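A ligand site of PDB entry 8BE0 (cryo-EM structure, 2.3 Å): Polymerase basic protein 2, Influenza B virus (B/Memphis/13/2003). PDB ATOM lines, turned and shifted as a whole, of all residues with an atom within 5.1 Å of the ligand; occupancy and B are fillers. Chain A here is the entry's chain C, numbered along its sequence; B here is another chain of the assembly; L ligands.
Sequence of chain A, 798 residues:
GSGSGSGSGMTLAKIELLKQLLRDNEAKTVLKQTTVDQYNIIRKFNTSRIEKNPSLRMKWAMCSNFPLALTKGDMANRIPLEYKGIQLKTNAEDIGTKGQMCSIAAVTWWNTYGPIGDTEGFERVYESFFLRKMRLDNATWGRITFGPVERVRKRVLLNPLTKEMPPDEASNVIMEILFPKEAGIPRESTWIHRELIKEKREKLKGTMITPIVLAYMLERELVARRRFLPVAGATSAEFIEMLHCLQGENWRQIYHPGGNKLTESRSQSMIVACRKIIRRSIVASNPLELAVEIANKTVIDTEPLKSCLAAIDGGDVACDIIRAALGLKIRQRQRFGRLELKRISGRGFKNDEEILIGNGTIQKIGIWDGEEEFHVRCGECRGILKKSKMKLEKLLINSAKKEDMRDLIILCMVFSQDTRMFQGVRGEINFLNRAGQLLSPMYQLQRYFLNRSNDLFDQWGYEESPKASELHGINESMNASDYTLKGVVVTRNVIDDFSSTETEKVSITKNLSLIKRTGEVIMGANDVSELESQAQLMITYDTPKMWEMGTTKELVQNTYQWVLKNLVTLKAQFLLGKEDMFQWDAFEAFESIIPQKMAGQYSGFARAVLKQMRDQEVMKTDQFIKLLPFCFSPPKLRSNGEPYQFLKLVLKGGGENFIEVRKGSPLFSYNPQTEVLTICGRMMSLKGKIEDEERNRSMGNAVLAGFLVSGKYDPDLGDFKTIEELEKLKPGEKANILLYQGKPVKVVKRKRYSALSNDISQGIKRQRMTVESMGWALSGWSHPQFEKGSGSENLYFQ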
ATOM      1  N   SER A 267      22.460 -32.098 -13.988  1.00  0.00           N
ATOM      2  CA  SER A 267      22.556 -30.646 -14.007  1.00  0.00           C
ATOM      3  C   SER A 267      23.599 -30.148 -13.016  1.00  0.00           C
ATOM      4  O   SER A 267      24.405 -29.267 -13.331  1.00  0.00           O
ATOM      5  CB  SER A 267      21.185 -30.031 -13.710  1.00  0.00           C
ATOM      6  OG  SER A 267      21.239 -28.616 -13.742  1.00  0.00           O
ATOM      7  N   GLN A 268      23.588 -30.704 -11.800  1.00  0.00           N
ATOM      8  CA  GLN A 268      24.575 -30.286 -10.799  1.00  0.00           C
ATOM      9  C   GLN A 268      25.991 -30.620 -11.258  1.00  0.00           C
ATOM     10  O   GLN A 268      26.908 -29.794 -11.107  1.00  0.00           O
ATOM     11  CB  GLN A 268      24.257 -30.960  -9.466  1.00  0.00           C
ATOM     12  CG  GLN A 268      25.045 -30.428  -8.282  1.00  0.00           C
ATOM     13  CD  GLN A 268      26.300 -31.236  -7.999  1.00  0.00           C
ATOM     14  OE1 GLN A 268      26.550 -32.266  -8.624  1.00  0.00           O
ATOM     15  NE2 GLN A 268      27.093 -30.769  -7.042  1.00  0.00           N
ATOM     16  N   ILE A 271      27.069 -28.209 -13.921  1.00  0.00           N
ATOM     17  CA  ILE A 271      27.384 -26.915 -13.328  1.00  0.00           C
ATOM     18  C   ILE A 271      28.789 -26.940 -12.722  1.00  0.00           C
ATOM     19  O   ILE A 271      29.584 -26.009 -12.927  1.00  0.00           O
ATOM     20  CB  ILE A 271      26.335 -26.530 -12.278  1.00  0.00           C
ATOM     21  CG1 ILE A 271      25.012 -26.171 -12.957  1.00  0.00           C
ATOM     22  CG2 ILE A 271      26.826 -25.367 -11.421  1.00  0.00           C
ATOM     23  CD1 ILE A 271      23.825 -26.140 -12.025  1.00  0.00           C
ATOM     24  N   ARG A 275      31.949 -24.674 -14.061  1.00  0.00           N
ATOM     25  CA  ARG A 275      32.660 -23.769 -13.159  1.00  0.00           C
ATOM     26  C   ARG A 275      34.153 -24.076 -13.137  1.00  0.00           C
ATOM     27  O   ARG A 275      34.982 -23.157 -13.197  1.00  0.00           O
ATOM     28  CB  ARG A 275      32.072 -23.855 -11.751  1.00  0.00           C
ATOM     29  CG  ARG A 275      30.721 -23.200 -11.620  1.00  0.00           C
ATOM     30  CD  ARG A 275      30.206 -23.280 -10.195  1.00  0.00           C
ATOM     31  NE  ARG A 275      28.885 -22.669 -10.053  1.00  0.00           N
ATOM     32  CZ  ARG A 275      28.211 -22.617  -8.920  1.00  0.00           C
ATOM     33  NH1 ARG A 275      28.694 -23.115  -7.797  1.00  0.00           N
ATOM     34  NH2 ARG A 275      27.018 -22.039  -8.906  1.00  0.00           N
ATOM     35  N   GLY A 314      18.573 -25.790 -18.047  1.00  0.00           N
ATOM     36  CA  GLY A 314      18.948 -25.121 -16.816  1.00  0.00           C
ATOM     37  C   GLY A 314      20.453 -24.939 -16.732  1.00  0.00           C
ATOM     38  O   GLY A 314      21.183 -25.189 -17.689  1.00  0.00           O
ATOM     39  N   GLY A 315      20.895 -24.508 -15.552  1.00  0.00           N
ATOM     40  CA  GLY A 315      22.300 -24.291 -15.290  1.00  0.00           C
ATOM     41  C   GLY A 315      22.560 -23.021 -14.520  1.00  0.00           C
ATOM     42  O   GLY A 315      21.696 -22.558 -13.761  1.00  0.00           O
ATOM     43  N   ASP A 316      23.742 -22.440 -14.692  1.00  0.00           N
ATOM     44  CA  ASP A 316      24.125 -21.198 -14.026  1.00  0.00           C
ATOM     45  C   ASP A 316      24.890 -20.346 -15.032  1.00  0.00           C
ATOM     46  O   ASP A 316      24.892 -20.622 -16.231  1.00  0.00           O
ATOM     47  CB  ASP A 316      24.932 -21.489 -12.759  1.00  0.00           C
ATOM     48  CG  ASP A 316      26.256 -22.169 -13.047  1.00  0.00           C
ATOM     49  OD1 ASP A 316      26.275 -23.087 -13.900  1.00  0.00           O
ATOM     50  OD2 ASP A 316      27.271 -21.785 -12.440  1.00  0.00           O
ATOM     51  N   ARG A 333      18.048 -19.837 -16.952  1.00  0.00           N
ATOM     52  CA  ARG A 333      17.255 -20.427 -15.890  1.00  0.00           C
ATOM     53  C   ARG A 333      18.089 -20.531 -14.617  1.00  0.00           C
ATOM     54  O   ARG A 333      19.298 -20.779 -14.657  1.00  0.00           O
ATOM     55  CB  ARG A 333      16.753 -21.815 -16.281  1.00  0.00           C
ATOM     56  CG  ARG A 333      15.410 -21.830 -17.004  1.00  0.00           C
ATOM     57  CD  ARG A 333      14.731 -23.184 -16.863  1.00  0.00           C
ATOM     58  NE  ARG A 333      13.545 -23.309 -17.704  1.00  0.00           N
ATOM     59  CZ  ARG A 333      12.691 -24.322 -17.659  1.00  0.00           C
ATOM     60  NH1 ARG A 333      12.850 -25.321 -16.810  1.00  0.00           N
ATOM     61  NH2 ARG A 333      11.647 -24.335 -18.489  1.00  0.00           N
ATOM     62  N   GLN A 334      17.416 -20.325 -13.481  1.00  0.00           N
ATOM     63  CA  GLN A 334      18.021 -20.433 -12.173  1.00  0.00           C
ATOM     64  C   GLN A 334      17.103 -21.261 -11.284  1.00  0.00           C
ATOM     65  O   GLN A 334      15.888 -21.243 -11.436  1.00  0.00           O
ATOM     66  CB  GLN A 334      18.261 -19.057 -11.538  1.00  0.00           C
ATOM     67  CG  GLN A 334      19.518 -18.362 -12.031  1.00  0.00           C
ATOM     68  CD  GLN A 334      19.528 -16.894 -11.693  1.00  0.00           C
ATOM     69  OE1 GLN A 334      18.830 -16.446 -10.782  1.00  0.00           O
ATOM     70  NE2 GLN A 334      20.332 -16.124 -12.413  1.00  0.00           N
ATOM     71  N   ARG A 335      17.719 -21.996 -10.355  1.00  0.00           N
ATOM     72  CA  ARG A 335      16.987 -22.862  -9.434  1.00  0.00           C
ATOM     73  C   ARG A 335      17.254 -22.407  -8.011  1.00  0.00           C
ATOM     74  O   ARG A 335      18.402 -22.176  -7.637  1.00  0.00           O
ATOM     75  CB  ARG A 335      17.416 -24.319  -9.625  1.00  0.00           C
ATOM     76  CG  ARG A 335      16.655 -25.308  -8.756  1.00  0.00           C
ATOM     77  CD  ARG A 335      15.249 -25.534  -9.262  1.00  0.00           C
ATOM     78  NE  ARG A 335      15.236 -26.143 -10.592  1.00  0.00           N
ATOM     79  CZ  ARG A 335      15.550 -27.404 -10.847  1.00  0.00           C
ATOM     80  NH1 ARG A 335      15.914 -28.230  -9.882  1.00  0.00           N
ATOM     81  NH2 ARG A 335      15.473 -27.847 -12.095  1.00  0.00           N
ATOM     82  N   PHE A 336      16.183 -22.277  -7.230  1.00  0.00           N
ATOM     83  CA  PHE A 336      16.267 -21.930  -5.814  1.00  0.00           C
ATOM     84  C   PHE A 336      15.510 -22.965  -4.986  1.00  0.00           C
ATOM     85  O   PHE A 336      14.702 -22.631  -4.119  1.00  0.00           O
ATOM     86  CB  PHE A 336      15.741 -20.525  -5.562  1.00  0.00           C
ATOM     87  CG  PHE A 336      15.911 -20.066  -4.140  1.00  0.00           C
ATOM     88  CD1 PHE A 336      17.175 -19.953  -3.587  1.00  0.00           C
ATOM     89  CD2 PHE A 336      14.813 -19.772  -3.355  1.00  0.00           C
ATOM     90  CE1 PHE A 336      17.345 -19.539  -2.279  1.00  0.00           C
ATOM     91  CE2 PHE A 336      14.974 -19.360  -2.052  1.00  0.00           C
ATOM     92  CZ  PHE A 336      16.242 -19.244  -1.507  1.00  0.00           C
ATOM     93  N   ARG A 343      15.567 -15.260 -16.096  1.00  0.00           N
ATOM     94  CA  ARG A 343      15.892 -13.841 -16.190  1.00  0.00           C
ATOM     95  C   ARG A 343      15.091 -13.199 -17.323  1.00  0.00           C
ATOM     96  O   ARG A 343      14.966 -13.767 -18.419  1.00  0.00           O
ATOM     97  CB  ARG A 343      17.392 -13.666 -16.422  1.00  0.00           C
ATOM     98  CG  ARG A 343      17.842 -12.338 -17.038  1.00  0.00           C
ATOM     99  CD  ARG A 343      17.740 -11.184 -16.048  1.00  0.00           C
ATOM    100  NE  ARG A 343      18.481 -11.398 -14.809  1.00  0.00           N
ATOM    101  CZ  ARG A 343      19.759 -11.741 -14.720  1.00  0.00           C
ATOM    102  NH1 ARG A 343      20.546 -11.792 -15.782  1.00  0.00           N
ATOM    103  NH2 ARG A 343      20.282 -12.006 -13.517  1.00  0.00           N
ATOM    104  N   GLY A 348      22.546  -8.652 -11.682  1.00  0.00           N
ATOM    105  CA  GLY A 348      22.774  -8.622 -10.249  1.00  0.00           C
ATOM    106  C   GLY A 348      24.235  -8.901  -9.920  1.00  0.00           C
ATOM    107  O   GLY A 348      24.935  -9.576 -10.671  1.00  0.00           O
ATOM    108  N   LYS A 350      26.716 -10.085  -6.491  1.00  0.00           N
ATOM    109  CA  LYS A 350      26.703 -10.696  -5.167  1.00  0.00           C
ATOM    110  C   LYS A 350      27.812 -10.089  -4.313  1.00  0.00           C
ATOM    111  O   LYS A 350      28.962  -9.973  -4.774  1.00  0.00           O
ATOM    112  CB  LYS A 350      26.871 -12.213  -5.266  1.00  0.00           C
ATOM    113  CG  LYS A 350      26.617 -12.961  -3.979  1.00  0.00           C
ATOM    114  CD  LYS A 350      26.812 -14.457  -4.187  1.00  0.00           C
ATOM    115  CE  LYS A 350      26.654 -15.234  -2.885  1.00  0.00           C
ATOM    116  NZ  LYS A 350      26.912 -16.685  -3.078  1.00  0.00           N
ATOM    117  N   TRP A 368      22.421  -9.869  -3.175  1.00  0.00           N
ATOM    118  CA  TRP A 368      22.426  -9.530  -4.590  1.00  0.00           C
ATOM    119  C   TRP A 368      21.848  -8.130  -4.773  1.00  0.00           C
ATOM    120  O   TRP A 368      20.705  -7.875  -4.398  1.00  0.00           O
ATOM    121  CB  TRP A 368      21.624 -10.560  -5.385  1.00  0.00           C
ATOM    122  CG  TRP A 368      22.284 -11.903  -5.435  1.00  0.00           C
ATOM    123  CD1 TRP A 368      22.193 -12.889  -4.507  1.00  0.00           C
ATOM    124  CD2 TRP A 368      23.121 -12.411  -6.478  1.00  0.00           C
ATOM    125  NE1 TRP A 368      22.932 -13.981  -4.893  1.00  0.00           N
ATOM    126  CE2 TRP A 368      23.512 -13.717  -6.101  1.00  0.00           C
ATOM    127  CE3 TRP A 368      23.588 -11.886  -7.687  1.00  0.00           C
ATOM    128  CZ2 TRP A 368      24.336 -14.497  -6.902  1.00  0.00           C
ATOM    129  CZ3 TRP A 368      24.408 -12.669  -8.479  1.00  0.00           C
ATOM    130  CH2 TRP A 368      24.782 -13.964  -8.082  1.00  0.00           C
ATOM    131  N   GLU A 372      16.256  -6.548 -10.792  1.00  0.00           N
ATOM    132  CA  GLU A 372      16.160  -7.709 -11.660  1.00  0.00           C
ATOM    133  C   GLU A 372      14.713  -8.139 -11.815  1.00  0.00           C
ATOM    134  O   GLU A 372      13.880  -7.943 -10.921  1.00  0.00           O
ATOM    135  CB  GLU A 372      17.012  -8.866 -11.117  1.00  0.00           C
ATOM    136  CG  GLU A 372      18.360  -8.433 -10.557  1.00  0.00           C
ATOM    137  CD  GLU A 372      19.305  -9.581 -10.321  1.00  0.00           C
ATOM    138  OE1 GLU A 372      19.471 -10.415 -11.232  1.00  0.00           O
ATOM    139  OE2 GLU A 372      19.885  -9.660  -9.217  1.00  0.00           O
ATOM    140  N   PHE A 374      12.286 -11.506 -13.021  1.00  0.00           N
ATOM    141  CA  PHE A 374      12.327 -12.958 -13.160  1.00  0.00           C
ATOM    142  C   PHE A 374      10.942 -13.517 -13.430  1.00  0.00           C
ATOM    143  O   PHE A 374       9.981 -13.179 -12.748  1.00  0.00           O
ATOM    144  CB  PHE A 374      12.909 -13.616 -11.907  1.00  0.00           C
ATOM    145  CG  PHE A 374      14.373 -13.373 -11.711  1.00  0.00           C
ATOM    146  CD1 PHE A 374      15.300 -14.023 -12.502  1.00  0.00           C
ATOM    147  CD2 PHE A 374      14.829 -12.500 -10.739  1.00  0.00           C
ATOM    148  CE1 PHE A 374      16.653 -13.811 -12.329  1.00  0.00           C
ATOM    149  CE2 PHE A 374      16.174 -12.282 -10.555  1.00  0.00           C
ATOM    150  CZ  PHE A 374      17.093 -12.935 -11.352  1.00  0.00           C
ATOM    151  N   LYS A 387      12.564  -7.507  -8.360  1.00  0.00           N
ATOM    152  CA  LYS A 387      13.371  -7.480  -7.144  1.00  0.00           C
ATOM    153  C   LYS A 387      14.380  -6.348  -7.240  1.00  0.00           C
ATOM    154  O   LYS A 387      14.823  -5.966  -8.328  1.00  0.00           O
ATOM    155  CB  LYS A 387      14.093  -8.823  -6.946  1.00  0.00           C
ATOM    156  CG  LYS A 387      15.225  -8.811  -5.927  1.00  0.00           C
ATOM    157  CD  LYS A 387      16.005 -10.116  -5.972  1.00  0.00           C
ATOM    158  CE  LYS A 387      17.179 -10.086  -5.008  1.00  0.00           C
ATOM    159  NZ  LYS A 387      18.108  -8.952  -5.288  1.00  0.00           N
ATOM    160  N   PHE A 415      13.743 -15.432  -1.689  1.00  0.00           N
ATOM    161  CA  PHE A 415      14.694 -15.266  -2.783  1.00  0.00           C
ATOM    162  C   PHE A 415      15.094 -13.812  -2.955  1.00  0.00           C
ATOM    163  O   PHE A 415      16.209 -13.522  -3.422  1.00  0.00           O
ATOM    164  CB  PHE A 415      14.090 -15.821  -4.073  1.00  0.00           C
ATOM    165  CG  PHE A 415      14.870 -15.469  -5.310  1.00  0.00           C
ATOM    166  CD1 PHE A 415      15.901 -16.275  -5.752  1.00  0.00           C
ATOM    167  CD2 PHE A 415      14.555 -14.327  -6.037  1.00  0.00           C
ATOM    168  CE1 PHE A 415      16.604 -15.962  -6.889  1.00  0.00           C
ATOM    169  CE2 PHE A 415      15.267 -14.000  -7.176  1.00  0.00           C
ATOM    170  CZ  PHE A 415      16.294 -14.822  -7.602  1.00  0.00           C
ATOM    171  N   GLN A 417      15.692 -11.653  -0.633  1.00  0.00           N
ATOM    172  CA  GLN A 417      16.561 -11.191   0.456  1.00  0.00           C
ATOM    173  C   GLN A 417      16.036  -9.883   1.040  1.00  0.00           C
ATOM    174  O   GLN A 417      16.808  -8.970   1.342  1.00  0.00           O
ATOM    175  CB  GLN A 417      18.002 -11.039  -0.019  1.00  0.00           C
ATOM    176  CG  GLN A 417      18.638 -12.317  -0.521  1.00  0.00           C
ATOM    177  CD  GLN A 417      20.006 -12.081  -1.132  1.00  0.00           C
ATOM    178  OE1 GLN A 417      20.221 -11.099  -1.830  1.00  0.00           O
ATOM    179  NE2 GLN A 417      20.935 -12.988  -0.866  1.00  0.00           N
ATOM    180  N   SER A 440      24.475 -23.432   3.068  1.00  0.00           N
ATOM    181  CA  SER A 440      24.035 -22.268   2.297  1.00  0.00           C
ATOM    182  C   SER A 440      22.974 -21.494   3.069  1.00  0.00           C
ATOM    183  O   SER A 440      21.889 -22.038   3.318  1.00  0.00           O
ATOM    184  CB  SER A 440      23.484 -22.713   0.948  1.00  0.00           C
ATOM    185  OG  SER A 440      23.166 -21.611   0.131  1.00  0.00           O
ATOM    186  N   MET A 442      20.818 -19.138   2.389  1.00  0.00           N
ATOM    187  CA  MET A 442      19.533 -18.841   1.775  1.00  0.00           C
ATOM    188  C   MET A 442      18.644 -20.076   1.749  1.00  0.00           C
ATOM    189  O   MET A 442      17.428 -19.975   1.964  1.00  0.00           O
ATOM    190  CB  MET A 442      19.733 -18.280   0.372  1.00  0.00           C
ATOM    191  CG  MET A 442      20.415 -16.919   0.320  1.00  0.00           C
ATOM    192  SD  MET A 442      19.681 -15.662   1.409  1.00  0.00           S
ATOM    193  CE  MET A 442      17.933 -15.878   1.090  1.00  0.00           C
ATOM    194  N   TYR A 443      19.215 -21.248   1.472  1.00  0.00           N
ATOM    195  CA  TYR A 443      18.424 -22.474   1.499  1.00  0.00           C
ATOM    196  C   TYR A 443      17.935 -22.771   2.908  1.00  0.00           C
ATOM    197  O   TYR A 443      16.804 -23.255   3.086  1.00  0.00           O
ATOM    198  CB  TYR A 443      19.240 -23.647   0.953  1.00  0.00           C
ATOM    199  CG  TYR A 443      19.189 -23.766  -0.545  1.00  0.00           C
ATOM    200  CD1 TYR A 443      18.175 -24.488  -1.170  1.00  0.00           C
ATOM    201  CD2 TYR A 443      20.155 -23.179  -1.340  1.00  0.00           C
ATOM    202  CE1 TYR A 443      18.130 -24.619  -2.538  1.00  0.00           C
ATOM    203  CE2 TYR A 443      20.115 -23.306  -2.716  1.00  0.00           C
ATOM    204  CZ  TYR A 443      19.104 -24.020  -3.311  1.00  0.00           C
ATOM    205  OH  TYR A 443      19.068 -24.136  -4.681  1.00  0.00           O
ATOM    206  N   SER A 529      30.287 -18.206  -9.683  1.00  0.00           N
ATOM    207  CA  SER A 529      30.494 -18.447  -8.263  1.00  0.00           C
ATOM    208  C   SER A 529      31.827 -19.144  -8.039  1.00  0.00           C
ATOM    209  O   SER A 529      32.226 -20.033  -8.792  1.00  0.00           O
ATOM    210  CB  SER A 529      29.354 -19.304  -7.704  1.00  0.00           C
ATOM    211  OG  SER A 529      29.568 -19.587  -6.333  1.00  0.00           O
ATOM    212  N   LEU A 531      32.464 -20.882  -5.331  1.00  0.00           N
ATOM    213  CA  LEU A 531      32.286 -22.000  -4.417  1.00  0.00           C
ATOM    214  C   LEU A 531      32.735 -23.305  -5.074  1.00  0.00           C
ATOM    215  O   LEU A 531      32.211 -23.696  -6.125  1.00  0.00           O
ATOM    216  CB  LEU A 531      30.828 -22.094  -3.999  1.00  0.00           C
ATOM    217  CG  LEU A 531      30.414 -23.341  -3.211  1.00  0.00           C
ATOM    218  CD1 LEU A 531      31.215 -23.464  -1.916  1.00  0.00           C
ATOM    219  CD2 LEU A 531      28.929 -23.311  -2.924  1.00  0.00           C
ATOM    220  P     A B   1      25.387 -27.868  -4.590  1.00  0.00           P
ATOM    221  OP1   A B   1      26.734 -27.516  -5.105  1.00  0.00           O
ATOM    222  OP2   A B   1      24.789 -29.187  -4.920  1.00  0.00           O
ATOM    223  O5'   A B   1      25.430 -27.714  -2.999  1.00  0.00           O
ATOM    224  C5'   A B   1      24.587 -28.511  -2.166  1.00  0.00           C
ATOM    225  C4'   A B   1      23.992 -27.708  -1.046  1.00  0.00           C
ATOM    226  O4'   A B   1      22.984 -26.807  -1.570  1.00  0.00           O
ATOM    227  C3'   A B   1      23.256 -28.505   0.021  1.00  0.00           C
ATOM    228  O3'   A B   1      24.124 -29.046   1.002  1.00  0.00           O
ATOM    229  C2'   A B   1      22.276 -27.482   0.589  1.00  0.00           C
ATOM    230  O2'   A B   1      22.924 -26.606   1.506  1.00  0.00           O
ATOM    231  C1'   A B   1      21.907 -26.694  -0.657  1.00  0.00           C
ATOM    232  N9    A B   1      20.695 -27.228  -1.307  1.00  0.00           N
ATOM    233  C8    A B   1      20.568 -27.706  -2.595  1.00  0.00           C
ATOM    234  N7    A B   1      19.360 -28.109  -2.890  1.00  0.00           N
ATOM    235  C5    A B   1      18.639 -27.885  -1.724  1.00  0.00           C
ATOM    236  C6    A B   1      17.287 -28.103  -1.397  1.00  0.00           C
ATOM    237  N6    A B   1      16.397 -28.610  -2.241  1.00  0.00           N
ATOM    238  N1    A B   1      16.883 -27.762  -0.151  1.00  0.00           N
ATOM    239  C2    A B   1      17.777 -27.244   0.699  1.00  0.00           C
ATOM    240  N3    A B   1      19.075 -26.995   0.501  1.00  0.00           N
ATOM    241  C4    A B   1      19.442 -27.341  -0.743  1.00  0.00           C
HETATM  242  N1  LIG L   1      21.476 -13.466 -10.529  1.00  0.00           N
HETATM  243  O1  LIG L   1      19.453 -12.312  -6.534  1.00  0.00           O
HETATM  244  C1  LIG L   1      19.905 -13.179  -7.286  1.00  0.00           C
HETATM  245  C2  LIG L   1      19.893 -14.460  -6.940  1.00  0.00           C
HETATM  246  N2  LIG L   1      19.453 -15.072  -5.848  1.00  0.00           N
HETATM  247  C3  LIG L   1      18.824 -14.438  -4.671  1.00  0.00           C
HETATM  248  C4  LIG L   1      19.671 -16.386  -5.983  1.00  0.00           C
HETATM  249  N3  LIG L   1      20.247 -16.568  -7.171  1.00  0.00           N
HETATM  250  C5  LIG L   1      20.398 -15.390  -7.764  1.00  0.00           C
HETATM  251  N4  LIG L   1      20.919 -15.056  -8.950  1.00  0.00           N
HETATM  252  C6  LIG L   1      20.956 -13.787  -9.349  1.00  0.00           C
HETATM  253  N5  LIG L   1      20.449 -12.794  -8.513  1.00  0.00           N
HETATM  254  O2  LIG L   1      21.240 -19.487  -9.531  1.00  0.00           O
HETATM  255  C7  LIG L   1      20.662 -17.871  -7.738  1.00  0.00           C
HETATM  256  C8  LIG L   1      22.152 -17.982  -7.936  1.00  0.00           C
HETATM  257  C9  LIG L   1      22.108 -19.396  -8.401  1.00  0.00           C
HETATM  258  C10 LIG L   1      21.414 -19.983  -7.191  1.00  0.00           C
HETATM  259  C11 LIG L   1      22.396 -20.008  -6.014  1.00  0.00           C
HETATM  260  O3  LIG L   1      20.387 -19.001  -6.856  1.00  0.00           O
HETATM  261  O4  LIG L   1      22.580 -17.097  -8.983  1.00  0.00           O
HETATM  262  P1  LIG L   1      23.071 -18.541  -3.934  1.00  0.00           P
HETATM  263  O5  LIG L   1      23.567 -19.744  -3.234  1.00  0.00           O
HETATM  264  O6  LIG L   1      22.424 -17.477  -3.141  1.00  0.00           O
HETATM  265  O7  LIG L   1      24.273 -17.867  -4.775  1.00  0.00           O
HETATM  266  O8  LIG L   1      22.044 -18.977  -5.094  1.00  0.00           O
HETATM  267  P2  LIG L   1      25.344 -18.730  -5.638  1.00  0.00           P
HETATM  268  O9  LIG L   1      26.697 -18.253  -5.297  1.00  0.00           O
HETATM  269  O10 LIG L   1      24.907 -18.763  -7.049  1.00  0.00           O
HETATM  270  O11 LIG L   1      25.187 -20.219  -5.044  1.00  0.00           O
HETATM  271  P3  LIG L   1      26.394 -21.260  -5.191  1.00  0.00           P
HETATM  272  O12 LIG L   1      26.794 -21.327  -6.616  1.00  0.00           O
HETATM  273  O13 LIG L   1      27.413 -20.966  -4.164  1.00  0.00           O
HETATM  274  O14 LIG L   1      25.687 -22.650  -4.816  1.00  0.00           O
HETATM  275  C12 LIG L   1      24.449 -23.000  -5.453  1.00  0.00           C
HETATM  276  C13 LIG L   1      23.942 -24.345  -4.933  1.00  0.00           C
HETATM  277  O15 LIG L   1      22.711 -24.625  -5.633  1.00  0.00           O
HETATM  278  C14 LIG L   1      24.866 -25.441  -5.416  1.00  0.00           C
HETATM  279  O16 LIG L   1      24.358 -26.726  -5.039  1.00  0.00           O
HETATM  280  C15 LIG L   1      24.606 -25.193  -6.873  1.00  0.00           C
HETATM  281  O17 LIG L   1      25.190 -26.198  -7.709  1.00  0.00           O
HETATM  282  C16 LIG L   1      23.110 -25.337  -6.853  1.00  0.00           C
HETATM  283  N6  LIG L   1      22.508 -24.759  -8.077  1.00  0.00           N
HETATM  284  C17 LIG L   1      22.619 -23.489  -8.437  1.00  0.00           C
HETATM  285  N7  LIG L   1      21.960 -23.335  -9.587  1.00  0.00           N
HETATM  286  C18 LIG L   1      21.450 -24.505  -9.930  1.00  0.00           C
HETATM  287  C19 LIG L   1      20.727 -24.868 -10.988  1.00  0.00           C
HETATM  288  N8  LIG L   1      20.445 -23.906 -11.856  1.00  0.00           N
HETATM  289  N9  LIG L   1      20.301 -26.124 -11.156  1.00  0.00           N
HETATM  290  C20 LIG L   1      20.635 -27.081 -10.200  1.00  0.00           C
HETATM  291  N10 LIG L   1      21.404 -26.674  -9.100  1.00  0.00           N
HETATM  292  C21 LIG L   1      21.795 -25.397  -9.002  1.00  0.00           C
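P of A 1 of chain B is bonded to O16 of the ligand (1.6 Å).
O12 of the ligand lies within salt-bridge range of NH2 of Arg 275 (2.4 Å).
O of Gly 315 sits at hydrogen-bond distance from N8 of the ligand (2.6 Å).
NZ of Lys 350 lies within salt-bridge range of O9 of the ligand (2.7 Å).
A nitrogen (N4) of the ligand sits close to the side-chain amide oxygen of Gln 334 (3.1 Å).
A nitrogen (N5) of the ligand sits at hydrogen-bond distance from the side-chain carboxylate (OE2) of Glu 372, at 3.3 Å.
O12 of the ligand is in hydrogen-bond range of OG of Ser 529 (3.3 Å).
Ser 267 touches the ligand (OG to N9, 3.7 Å).
Ile 271 touches the ligand.
Arg 335 touches the ligand (CB to C19, 3.6 Å).
Arg 343 touches the ligand.
CB of Trp 368 touches O1 of the ligand, 3.0 Å away.
Lys 387 touches the ligand.
Phe 415 touches the ligand.
Ser 440 touches the ligand.
Tyr 443 touches the ligand.
Leu 531 touches the ligand (CD2 to O13, 3.1 Å).
Of the 26 residues printed, 17 come within 4 Å of the ligand.
The nearest printed residue that does not touch the ligand is Met 442 (4.04 Å).
The side-chain carboxylate (OD2) of Asp 316 is in salt-bridge range of the guanidinium group (NE) of Arg 275.
The backbone carbonyl oxygen (O) of Trp 368 sits at hydrogen-bond distance from the side-chain amino group (NZ) of Lys 387, 2.9 Å away.
The side-chain amide oxygen (OE1) of Gln 417 lies within hydrogen-bond range of the backbone NH (N) of Trp 368 (2.9 Å).
N of Leu 531 lies close to OG of Ser 529, 3.3 Å away.
N of Glu 372 lies within hydrogen-bond range of O of Lys 387.
OE1 of Glu 372 lies within salt-bridge range of NH2 of Arg 343.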
